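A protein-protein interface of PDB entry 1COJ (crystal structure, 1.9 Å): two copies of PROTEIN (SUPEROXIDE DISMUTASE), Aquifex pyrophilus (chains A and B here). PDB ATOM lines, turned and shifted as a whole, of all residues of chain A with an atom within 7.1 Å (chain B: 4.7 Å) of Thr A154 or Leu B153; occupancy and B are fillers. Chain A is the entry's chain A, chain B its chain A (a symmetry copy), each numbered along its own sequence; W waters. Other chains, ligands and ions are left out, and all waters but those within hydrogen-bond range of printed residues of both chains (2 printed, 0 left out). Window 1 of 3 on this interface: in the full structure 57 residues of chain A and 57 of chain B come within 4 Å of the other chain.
The backbone NH of Thr B154 lies within hydrogen-bond range of the side-chain sulfur of Met A76, at 3.5 Å. The backbone NH of Tyr B151 is in hydrogen-bond range of the backbone carbonyl oxygen of Asn A149 (2.9 Å). The side-chain hydroxyl of Thr B154 sits at hydrogen-bond distance from the side-chain amide nitrogen of Asn A152 (3.1 Å). The backbone NH of Thr A154 lies within hydrogen-bond range of the side-chain sulfur of Met B76, at 3.5 Å. ND2 of Asn B152 sits at hydrogen-bond distance from OG1 of Thr A154, at 3.1 Å. O of Leu B156 is in hydrogen-bond range of N of Gly A155 (3.0 Å). O of Leu A156 lies within hydrogen-bond range of N of Gly B155, at 3.0 Å.
The side-chain amide oxygen (OD1) of Asn A149 sits at hydrogen-bond distance from the side-chain hydroxyl (OG1) of Thr A72. OD1 of Asn A149 sits close to N of Phe A73 (3.5 Å). The side-chain carboxylate (OD2) of Asp A134 sits close to the backbone NH (N) of Phe A136 (3.2 Å). N of Leu A153 is in hydrogen-bond range of OD1 of Asn A143 (3.0 Å). The side-chain amide nitrogen (ND2) of Asn A152 sits at hydrogen-bond distance from the backbone carbonyl oxygen (O) of His A148 (2.9 Å). The backbone NH (N) of Leu B153 is in hydrogen-bond range of the side-chain amide oxygen (OD1) of Asn B143 (3.0 Å).
Among the printed residues, pairs that only touch across the chains: Thr A72 with Asn B143 (3.6 Å), Thr A72 with Tyr B151 (3.5 Å), Thr A72 with Leu B153 (3.97 Å), Met A76 with Leu B153 (3.9 Å), Phe A136 with Pro B158 (3.9 Å), Asn A152 with Asn B152 (3.2 Å), Leu A153 with Met B76 (3.9 Å), Leu A153 with Thr B154 (3.99 Å), Thr A154 with Leu B153 (3.99 Å), Thr A154 with Leu B156 (3.4 Å), Thr A154 with Pro B158 (3.5 Å), Gly A155 with Gly B155 (3.8 Å) and Leu A156 with Thr B154 (3.4 Å).
Printed residues of chain B within 4 Å of Thr A154: Met B76, Asn B152, Leu B153, Leu B156 and Pro B158. Of the printed residues of chain A, Leu B153 touches Thr A72 (3.97 Å), Met A76 (3.9 Å) and Thr A154 (3.99 Å). Printed residues of chain B within 4 Å of Asn A152: Asn B152 (3.2 Å) and Thr B154 (3.1 Å). Of the printed residues of chain B, Gly A155 touches Gly B155 and Leu B156. Printed residues of chain A within 4 Å of Asn B143: Thr A72. Leu B80 touches none of the printed residues of chain A.
Of the 11 printed residues of chain B, 9 touch a printed residue of chain A. Hydrophobic or aromatic side chains of chain B within 4 Å of the printed part of chain A: Met B76, Tyr B151, Leu B153 and Pro B158. Hydrophobic or aromatic side chains of chain A within 4 Å of the printed part of chain B: Met A76, Phe A136 and Leu A153. Among the printed residues, 20 pairs touch across the chains. Among the printed residues, no Asp or Glu carboxylate lies within 4 Å of a Lys or Arg side-chain nitrogen of the other chain.
Met A76 touches Leu B153, and with the chains exchanged Leu A153 touches Met B76. Asn B152 touches its own counterpart, Asn A152. Asn A152 touches Thr B154, and with the chains exchanged Thr A154 touches Asn B152. Gly A155 touches Leu B156, and with the chains exchanged Leu A156 touches Gly B155. Positions printed for both chains: 76, 143, 151, 152, 153, 154, 155 and 156. Of the 20 pairs that touch across the chains among the printed residues, 14 have their exchanged pair printed and touching as well.
Water W2 lies within hydrogen-bond range of OG1 of Thr B154 (2.8 Å), O of Leu A153 (2.9 Å) and OD1 of Asn A143 (3.0 Å). Water W1 lies within hydrogen-bond range of the side-chain hydroxyl of Thr A154 (2.8 Å), the backbone carbonyl oxygen of Leu B153 (2.9 Å) and the side-chain amide oxygen of Asn B143 (3.0 Å).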
ATOM      1  N   GLU A  71     -22.368  17.701   4.805  1.00  0.00           N
ATOM      2  CA  GLU A  71     -21.438  16.589   4.746  1.00  0.00           C
ATOM      3  C   GLU A  71     -21.820  15.587   5.830  1.00  0.00           C
ATOM      4  O   GLU A  71     -21.795  14.378   5.593  1.00  0.00           O
ATOM      5  CB  GLU A  71     -19.999  17.052   4.966  1.00  0.00           C
ATOM      6  CG  GLU A  71     -18.974  15.921   4.848  1.00  0.00           C
ATOM      7  CD  GLU A  71     -17.559  16.383   5.139  1.00  0.00           C
ATOM      8  OE1 GLU A  71     -17.386  17.192   6.071  1.00  0.00           O
ATOM      9  OE2 GLU A  71     -16.621  15.940   4.442  1.00  0.00           O
ATOM     10  N   THR A  72     -22.190  16.084   7.011  1.00  0.00           N
ATOM     11  CA  THR A  72     -22.574  15.208   8.113  1.00  0.00           C
ATOM     12  C   THR A  72     -23.900  14.511   7.814  1.00  0.00           C
ATOM     13  O   THR A  72     -24.078  13.337   8.140  1.00  0.00           O
ATOM     14  CB  THR A  72     -22.683  15.959   9.476  1.00  0.00           C
ATOM     15  OG1 THR A  72     -23.720  16.941   9.419  1.00  0.00           O
ATOM     16  CG2 THR A  72     -21.369  16.634   9.827  1.00  0.00           C
ATOM     17  N   PHE A  73     -24.816  15.226   7.164  1.00  0.00           N
ATOM     18  CA  PHE A  73     -26.121  14.671   6.815  1.00  0.00           C
ATOM     19  C   PHE A  73     -25.972  13.494   5.858  1.00  0.00           C
ATOM     20  O   PHE A  73     -26.496  12.402   6.108  1.00  0.00           O
ATOM     21  CB  PHE A  73     -27.013  15.740   6.173  1.00  0.00           C
ATOM     22  CG  PHE A  73     -28.402  15.256   5.848  1.00  0.00           C
ATOM     23  CD1 PHE A  73     -29.359  15.128   6.851  1.00  0.00           C
ATOM     24  CD2 PHE A  73     -28.740  14.894   4.543  1.00  0.00           C
ATOM     25  CE1 PHE A  73     -30.637  14.649   6.563  1.00  0.00           C
ATOM     26  CE2 PHE A  73     -30.011  14.414   4.242  1.00  0.00           C
ATOM     27  CZ  PHE A  73     -30.963  14.288   5.254  1.00  0.00           C
ATOM     28  N   TYR A  75     -23.026  11.849   4.898  1.00  0.00           N
ATOM     29  CA  TYR A  75     -22.117  10.797   5.330  1.00  0.00           C
ATOM     30  C   TYR A  75     -22.810   9.874   6.319  1.00  0.00           C
ATOM     31  O   TYR A  75     -22.660   8.653   6.244  1.00  0.00           O
ATOM     32  CB  TYR A  75     -20.839  11.376   5.938  1.00  0.00           C
ATOM     33  CG  TYR A  75     -19.786  10.327   6.224  1.00  0.00           C
ATOM     34  CD1 TYR A  75     -19.296   9.500   5.210  1.00  0.00           C
ATOM     35  CD2 TYR A  75     -19.291  10.150   7.512  1.00  0.00           C
ATOM     36  CE1 TYR A  75     -18.339   8.517   5.477  1.00  0.00           C
ATOM     37  CE2 TYR A  75     -18.335   9.172   7.792  1.00  0.00           C
ATOM     38  CZ  TYR A  75     -17.864   8.360   6.771  1.00  0.00           C
ATOM     39  OH  TYR A  75     -16.930   7.386   7.049  1.00  0.00           O
ATOM     40  N   MET A  76     -23.565  10.452   7.252  1.00  0.00           N
ATOM     41  CA  MET A  76     -24.291   9.642   8.223  1.00  0.00           C
ATOM     42  C   MET A  76     -25.376   8.855   7.501  1.00  0.00           C
ATOM     43  O   MET A  76     -25.673   7.718   7.862  1.00  0.00           O
ATOM     44  CB  MET A  76     -24.886  10.505   9.337  1.00  0.00           C
ATOM     45  CG  MET A  76     -23.868  10.947  10.379  1.00  0.00           C
ATOM     46  SD  MET A  76     -23.190   9.572  11.334  1.00  0.00           S
ATOM     47  CE  MET A  76     -21.691   9.167  10.414  1.00  0.00           C
ATOM     48  N   LEU A 133     -22.323   1.247  21.966  1.00  0.00           N
ATOM     49  CA  LEU A 133     -21.426   1.354  23.104  1.00  0.00           C
ATOM     50  C   LEU A 133     -20.879   2.777  23.200  1.00  0.00           C
ATOM     51  O   LEU A 133     -20.274   3.294  22.255  1.00  0.00           O
ATOM     52  CB  LEU A 133     -20.259   0.369  22.979  1.00  0.00           C
ATOM     53  CG  LEU A 133     -19.265   0.350  24.150  1.00  0.00           C
ATOM     54  CD1 LEU A 133     -19.888  -0.345  25.355  1.00  0.00           C
ATOM     55  CD2 LEU A 133     -17.996  -0.365  23.737  1.00  0.00           C
ATOM     56  N   ASP A 134     -21.130   3.412  24.335  1.00  0.00           N
ATOM     57  CA  ASP A 134     -20.657   4.764  24.595  1.00  0.00           C
ATOM     58  C   ASP A 134     -19.205   4.618  25.065  1.00  0.00           C
ATOM     59  O   ASP A 134     -18.953   4.135  26.172  1.00  0.00           O
ATOM     60  CB  ASP A 134     -21.538   5.394  25.680  1.00  0.00           C
ATOM     61  CG  ASP A 134     -20.952   6.676  26.263  1.00  0.00           C
ATOM     62  OD1 ASP A 134     -21.249   6.965  27.437  1.00  0.00           O
ATOM     63  OD2 ASP A 134     -20.208   7.394  25.564  1.00  0.00           O
ATOM     64  N   ILE A 135     -18.253   5.051  24.243  1.00  0.00           N
ATOM     65  CA  ILE A 135     -16.840   4.916  24.597  1.00  0.00           C
ATOM     66  C   ILE A 135     -16.400   5.719  25.813  1.00  0.00           C
ATOM     67  O   ILE A 135     -15.357   5.433  26.397  1.00  0.00           O
ATOM     68  CB  ILE A 135     -15.899   5.256  23.421  1.00  0.00           C
ATOM     69  CG1 ILE A 135     -16.078   6.715  22.992  1.00  0.00           C
ATOM     70  CG2 ILE A 135     -16.148   4.308  22.269  1.00  0.00           C
ATOM     71  CD1 ILE A 135     -14.991   7.221  22.065  1.00  0.00           C
ATOM     72  N   PHE A 136     -17.191   6.711  26.205  1.00  0.00           N
ATOM     73  CA  PHE A 136     -16.839   7.539  27.351  1.00  0.00           C
ATOM     74  C   PHE A 136     -17.201   6.920  28.695  1.00  0.00           C
ATOM     75  O   PHE A 136     -16.552   7.214  29.699  1.00  0.00           O
ATOM     76  CB  PHE A 136     -17.435   8.940  27.208  1.00  0.00           C
ATOM     77  CG  PHE A 136     -17.001   9.653  25.951  1.00  0.00           C
ATOM     78  CD1 PHE A 136     -15.671  10.033  25.767  1.00  0.00           C
ATOM     79  CD2 PHE A 136     -17.917   9.914  24.937  1.00  0.00           C
ATOM     80  CE1 PHE A 136     -15.264  10.661  24.592  1.00  0.00           C
ATOM     81  CE2 PHE A 136     -17.518  10.539  23.761  1.00  0.00           C
ATOM     82  CZ  PHE A 136     -16.188  10.913  23.588  1.00  0.00           C
ATOM     83  N   ASN A 143     -29.553   5.447  21.741  1.00  0.00           N
ATOM     84  CA  ASN A 143     -29.442   6.804  21.218  1.00  0.00           C
ATOM     85  C   ASN A 143     -30.476   7.015  20.107  1.00  0.00           C
ATOM     86  O   ASN A 143     -30.452   6.328  19.086  1.00  0.00           O
ATOM     87  CB  ASN A 143     -28.016   7.000  20.675  1.00  0.00           C
ATOM     88  CG  ASN A 143     -27.753   8.400  20.111  1.00  0.00           C
ATOM     89  OD1 ASN A 143     -26.797   8.585  19.357  1.00  0.00           O
ATOM     90  ND2 ASN A 143     -28.553   9.392  20.505  1.00  0.00           N
ATOM     91  N   HIS A 148     -30.433  12.000  10.219  1.00  0.00           N
ATOM     92  CA  HIS A 148     -29.126  11.350  10.105  1.00  0.00           C
ATOM     93  C   HIS A 148     -28.055  12.037  10.950  1.00  0.00           C
ATOM     94  O   HIS A 148     -27.177  11.373  11.499  1.00  0.00           O
ATOM     95  CB  HIS A 148     -28.636  11.338   8.650  1.00  0.00           C
ATOM     96  CG  HIS A 148     -29.614  10.763   7.674  1.00  0.00           C
ATOM     97  ND1 HIS A 148     -30.313   9.601   7.904  1.00  0.00           N
ATOM     98  CD2 HIS A 148     -29.992  11.187   6.439  1.00  0.00           C
ATOM     99  CE1 HIS A 148     -31.085   9.331   6.865  1.00  0.00           C
ATOM    100  NE2 HIS A 148     -30.906  10.281   5.962  1.00  0.00           N
ATOM    101  N   ASN A 149     -28.154  13.359  11.067  1.00  0.00           N
ATOM    102  CA  ASN A 149     -27.169  14.161  11.794  1.00  0.00           C
ATOM    103  C   ASN A 149     -27.716  15.012  12.944  1.00  0.00           C
ATOM    104  O   ASN A 149     -27.158  16.067  13.267  1.00  0.00           O
ATOM    105  CB  ASN A 149     -26.418  15.064  10.801  1.00  0.00           C
ATOM    106  CG  ASN A 149     -27.338  16.064  10.072  1.00  0.00           C
ATOM    107  OD1 ASN A 149     -26.864  16.943   9.361  1.00  0.00           O
ATOM    108  ND2 ASN A 149     -28.639  15.942  10.266  1.00  0.00           N
ATOM    109  N   TYR A 151     -28.865  14.754  16.978  1.00  0.00           N
ATOM    110  CA  TYR A 151     -28.885  14.066  18.282  1.00  0.00           C
ATOM    111  C   TYR A 151     -27.915  12.888  18.416  1.00  0.00           C
ATOM    112  O   TYR A 151     -27.937  12.162  19.417  1.00  0.00           O
ATOM    113  CB  TYR A 151     -30.308  13.658  18.704  1.00  0.00           C
ATOM    114  CG  TYR A 151     -31.292  14.816  18.780  1.00  0.00           C
ATOM    115  CD1 TYR A 151     -32.657  14.615  18.554  1.00  0.00           C
ATOM    116  CD2 TYR A 151     -30.855  16.118  19.050  1.00  0.00           C
ATOM    117  CE1 TYR A 151     -33.561  15.685  18.589  1.00  0.00           C
ATOM    118  CE2 TYR A 151     -31.744  17.191  19.090  1.00  0.00           C
ATOM    119  CZ  TYR A 151     -33.096  16.974  18.853  1.00  0.00           C
ATOM    120  OH  TYR A 151     -33.972  18.042  18.836  1.00  0.00           O
ATOM    121  N   ASN A 152     -27.047  12.719  17.421  1.00  0.00           N
ATOM    122  CA  ASN A 152     -26.064  11.641  17.434  1.00  0.00           C
ATOM    123  C   ASN A 152     -25.097  11.888  18.577  1.00  0.00           C
ATOM    124  O   ASN A 152     -24.650  13.019  18.775  1.00  0.00           O
ATOM    125  CB  ASN A 152     -25.211  11.625  16.156  1.00  0.00           C
ATOM    126  CG  ASN A 152     -26.023  11.716  14.882  1.00  0.00           C
ATOM    127  OD1 ASN A 152     -26.804  12.642  14.696  1.00  0.00           O
ATOM    128  ND2 ASN A 152     -25.807  10.776  13.977  1.00  0.00           N
ATOM    129  N   LEU A 153     -24.758  10.837  19.316  1.00  0.00           N
ATOM    130  CA  LEU A 153     -23.783  10.971  20.384  1.00  0.00           C
ATOM    131  C   LEU A 153     -22.392  10.766  19.780  1.00  0.00           C
ATOM    132  O   LEU A 153     -22.163   9.815  19.023  1.00  0.00           O
ATOM    133  CB  LEU A 153     -24.023   9.938  21.487  1.00  0.00           C
ATOM    134  CG  LEU A 153     -25.228  10.123  22.410  1.00  0.00           C
ATOM    135  CD1 LEU A 153     -25.345   8.916  23.316  1.00  0.00           C
ATOM    136  CD2 LEU A 153     -25.090  11.390  23.238  1.00  0.00           C
ATOM    137  N   THR A 154     -21.486  11.692  20.064  1.00  0.00           N
ATOM    138  CA  THR A 154     -20.115  11.597  19.585  1.00  0.00           C
ATOM    139  C   THR A 154     -19.487  10.339  20.201  1.00  0.00           C
ATOM    140  O   THR A 154     -19.800   9.980  21.342  1.00  0.00           O
ATOM    141  CB  THR A 154     -19.299  12.838  20.047  1.00  0.00           C
ATOM    142  OG1 THR A 154     -19.772  14.010  19.374  1.00  0.00           O
ATOM    143  CG2 THR A 154     -17.822  12.665  19.752  1.00  0.00           C
ATOM    144  N   GLY A 155     -18.665   9.640  19.423  1.00  0.00           N
ATOM    145  CA  GLY A 155     -17.981   8.453  19.912  1.00  0.00           C
ATOM    146  C   GLY A 155     -18.725   7.132  19.984  1.00  0.00           C
ATOM    147  O   GLY A 155     -18.097   6.083  20.111  1.00  0.00           O
ATOM    148  N   LEU A 156     -20.046   7.166  19.876  1.00  0.00           N
ATOM    149  CA  LEU A 156     -20.857   5.954  19.961  1.00  0.00           C
ATOM    150  C   LEU A 156     -20.537   4.914  18.882  1.00  0.00           C
ATOM    151  O   LEU A 156     -20.478   5.239  17.697  1.00  0.00           O
ATOM    152  CB  LEU A 156     -22.350   6.321  19.902  1.00  0.00           C
ATOM    153  CG  LEU A 156     -23.365   5.211  20.198  1.00  0.00           C
ATOM    154  CD1 LEU A 156     -23.442   4.986  21.689  1.00  0.00           C
ATOM    155  CD2 LEU A 156     -24.732   5.587  19.673  1.00  0.00           C
ATOM    156  N   ILE A 157     -20.307   3.670  19.303  1.00  0.00           N
ATOM    157  CA  ILE A 157     -20.040   2.576  18.369  1.00  0.00           C
ATOM    158  C   ILE A 157     -21.383   1.853  18.226  1.00  0.00           C
ATOM    159  O   ILE A 157     -21.851   1.207  19.163  1.00  0.00           O
ATOM    160  CB  ILE A 157     -18.972   1.605  18.913  1.00  0.00           C
ATOM    161  CG1 ILE A 157     -17.679   2.367  19.214  1.00  0.00           C
ATOM    162  CG2 ILE A 157     -18.688   0.509  17.891  1.00  0.00           C
ATOM    163  CD1 ILE A 157     -16.624   1.530  19.899  1.00  0.00           C
ATOM    164  N   MET B  76     -23.605  15.370  26.120  1.00  0.00           N
ATOM    165  CA  MET B  76     -22.573  15.883  25.227  1.00  0.00           C
ATOM    166  C   MET B  76     -21.992  17.159  25.821  1.00  0.00           C
ATOM    167  O   MET B  76     -20.799  17.428  25.687  1.00  0.00           O
ATOM    168  CB  MET B  76     -23.123  16.131  23.821  1.00  0.00           C
ATOM    169  CG  MET B  76     -23.288  14.862  22.996  1.00  0.00           C
ATOM    170  SD  MET B  76     -21.718  14.056  22.614  1.00  0.00           S
ATOM    171  CE  MET B  76     -21.563  12.857  23.956  1.00  0.00           C
ATOM    172  N   LEU B  80     -18.012  16.969  26.088  1.00  0.00           N
ATOM    173  CA  LEU B  80     -17.281  17.939  25.279  1.00  0.00           C
ATOM    174  C   LEU B  80     -16.529  18.948  26.141  1.00  0.00           C
ATOM    175  O   LEU B  80     -15.391  19.300  25.833  1.00  0.00           O
ATOM    176  CB  LEU B  80     -18.228  18.633  24.295  1.00  0.00           C
ATOM    177  CG  LEU B  80     -18.390  18.017  22.893  1.00  0.00           C
ATOM    178  CD1 LEU B  80     -18.104  16.530  22.863  1.00  0.00           C
ATOM    179  CD2 LEU B  80     -19.782  18.320  22.364  1.00  0.00           C
ATOM    180  N   VAL B 141     -10.856  13.641  10.592  1.00  0.00           N
ATOM    181  CA  VAL B 141     -11.829  14.533   9.974  1.00  0.00           C
ATOM    182  C   VAL B 141     -12.168  15.695  10.901  1.00  0.00           C
ATOM    183  O   VAL B 141     -12.015  15.600  12.122  1.00  0.00           O
ATOM    184  CB  VAL B 141     -13.155  13.799   9.615  1.00  0.00           C
ATOM    185  CG1 VAL B 141     -12.894  12.642   8.658  1.00  0.00           C
ATOM    186  CG2 VAL B 141     -13.849  13.302  10.867  1.00  0.00           C
ATOM    187  N   ASN B 143     -15.066  17.900  12.281  1.00  0.00           N
ATOM    188  CA  ASN B 143     -16.511  17.837  12.464  1.00  0.00           C
ATOM    189  C   ASN B 143     -16.995  19.098  13.188  1.00  0.00           C
ATOM    190  O   ASN B 143     -16.590  19.369  14.319  1.00  0.00           O
ATOM    191  CB  ASN B 143     -16.842  16.580  13.286  1.00  0.00           C
ATOM    192  CG  ASN B 143     -18.341  16.378  13.535  1.00  0.00           C
ATOM    193  OD1 ASN B 143     -18.714  15.628  14.438  1.00  0.00           O
ATOM    194  ND2 ASN B 143     -19.197  16.993  12.719  1.00  0.00           N
ATOM    195  N   TYR B 151     -25.279  17.831  14.617  1.00  0.00           N
ATOM    196  CA  TYR B 151     -24.282  17.571  13.561  1.00  0.00           C
ATOM    197  C   TYR B 151     -23.112  16.674  13.973  1.00  0.00           C
ATOM    198  O   TYR B 151     -22.155  16.494  13.211  1.00  0.00           O
ATOM    199  CB  TYR B 151     -23.776  18.870  12.906  1.00  0.00           C
ATOM    200  CG  TYR B 151     -24.875  19.730  12.299  1.00  0.00           C
ATOM    201  CD1 TYR B 151     -24.734  21.119  12.212  1.00  0.00           C
ATOM    202  CD2 TYR B 151     -26.066  19.160  11.837  1.00  0.00           C
ATOM    203  CE1 TYR B 151     -25.757  21.918  11.687  1.00  0.00           C
ATOM    204  CE2 TYR B 151     -27.092  19.944  11.309  1.00  0.00           C
ATOM    205  CZ  TYR B 151     -26.938  21.323  11.240  1.00  0.00           C
ATOM    206  OH  TYR B 151     -27.973  22.108  10.770  1.00  0.00           O
ATOM    207  N   ASN B 152     -23.203  16.090  15.166  1.00  0.00           N
ATOM    208  CA  ASN B 152     -22.159  15.203  15.669  1.00  0.00           C
ATOM    209  C   ASN B 152     -22.111  13.971  14.785  1.00  0.00           C
ATOM    210  O   ASN B 152     -23.156  13.419  14.435  1.00  0.00           O
ATOM    211  CB  ASN B 152     -22.472  14.694  17.085  1.00  0.00           C
ATOM    212  CG  ASN B 152     -22.881  15.788  18.048  1.00  0.00           C
ATOM    213  OD1 ASN B 152     -23.822  16.531  17.795  1.00  0.00           O
ATOM    214  ND2 ASN B 152     -22.203  15.860  19.180  1.00  0.00           N
ATOM    215  N   LEU B 153     -20.908  13.526  14.440  1.00  0.00           N
ATOM    216  CA  LEU B 153     -20.769  12.311  13.655  1.00  0.00           C
ATOM    217  C   LEU B 153     -20.727  11.128  14.624  1.00  0.00           C
ATOM    218  O   LEU B 153     -20.000  11.152  15.625  1.00  0.00           O
ATOM    219  CB  LEU B 153     -19.488  12.335  12.817  1.00  0.00           C
ATOM    220  CG  LEU B 153     -19.430  13.262  11.602  1.00  0.00           C
ATOM    221  CD1 LEU B 153     -18.032  13.227  11.022  1.00  0.00           C
ATOM    222  CD2 LEU B 153     -20.445  12.846  10.551  1.00  0.00           C
ATOM    223  N   THR B 154     -21.553  10.124  14.361  1.00  0.00           N
ATOM    224  CA  THR B 154     -21.586   8.922  15.180  1.00  0.00           C
ATOM    225  C   THR B 154     -20.215   8.241  15.074  1.00  0.00           C
ATOM    226  O   THR B 154     -19.578   8.284  14.017  1.00  0.00           O
ATOM    227  CB  THR B 154     -22.672   7.942  14.650  1.00  0.00           C
ATOM    228  OG1 THR B 154     -23.975   8.492  14.870  1.00  0.00           O
ATOM    229  CG2 THR B 154     -22.583   6.597  15.344  1.00  0.00           C
ATOM    230  N   GLY B 155     -19.739   7.681  16.184  1.00  0.00           N
ATOM    231  CA  GLY B 155     -18.469   6.972  16.192  1.00  0.00           C
ATOM    232  C   GLY B 155     -17.171   7.756  16.262  1.00  0.00           C
ATOM    233  O   GLY B 155     -16.125   7.183  16.561  1.00  0.00           O
ATOM    234  N   LEU B 156     -17.228   9.059  16.019  1.00  0.00           N
ATOM    235  CA  LEU B 156     -16.031   9.898  16.032  1.00  0.00           C
ATOM    236  C   LEU B 156     -15.301   9.918  17.378  1.00  0.00           C
ATOM    237  O   LEU B 156     -15.916  10.133  18.421  1.00  0.00           O
ATOM    238  CB  LEU B 156     -16.397  11.333  15.617  1.00  0.00           C
ATOM    239  CG  LEU B 156     -15.245  12.310  15.356  1.00  0.00           C
ATOM    240  CD1 LEU B 156     -14.650  12.032  13.997  1.00  0.00           C
ATOM    241  CD2 LEU B 156     -15.739  13.739  15.406  1.00  0.00           C
ATOM    242  N   PRO B 158     -12.917  11.995  19.433  1.00  0.00           N
ATOM    243  CA  PRO B 158     -12.394  13.367  19.530  1.00  0.00           C
ATOM    244  C   PRO B 158     -10.952  13.490  19.993  1.00  0.00           C
ATOM    245  O   PRO B 158     -10.567  12.898  21.000  1.00  0.00           O
ATOM    246  CB  PRO B 158     -13.325  14.023  20.556  1.00  0.00           C
ATOM    247  CG  PRO B 158     -14.508  13.099  20.645  1.00  0.00           C
ATOM    248  CD  PRO B 158     -13.896  11.747  20.499  1.00  0.00           C
HETATM  249  O   HOH W   1     -18.946  13.655  16.727  1.00  0.00           O
HETATM  250  O   HOH W   2     -24.307   8.368  17.643  1.00  0.00           O
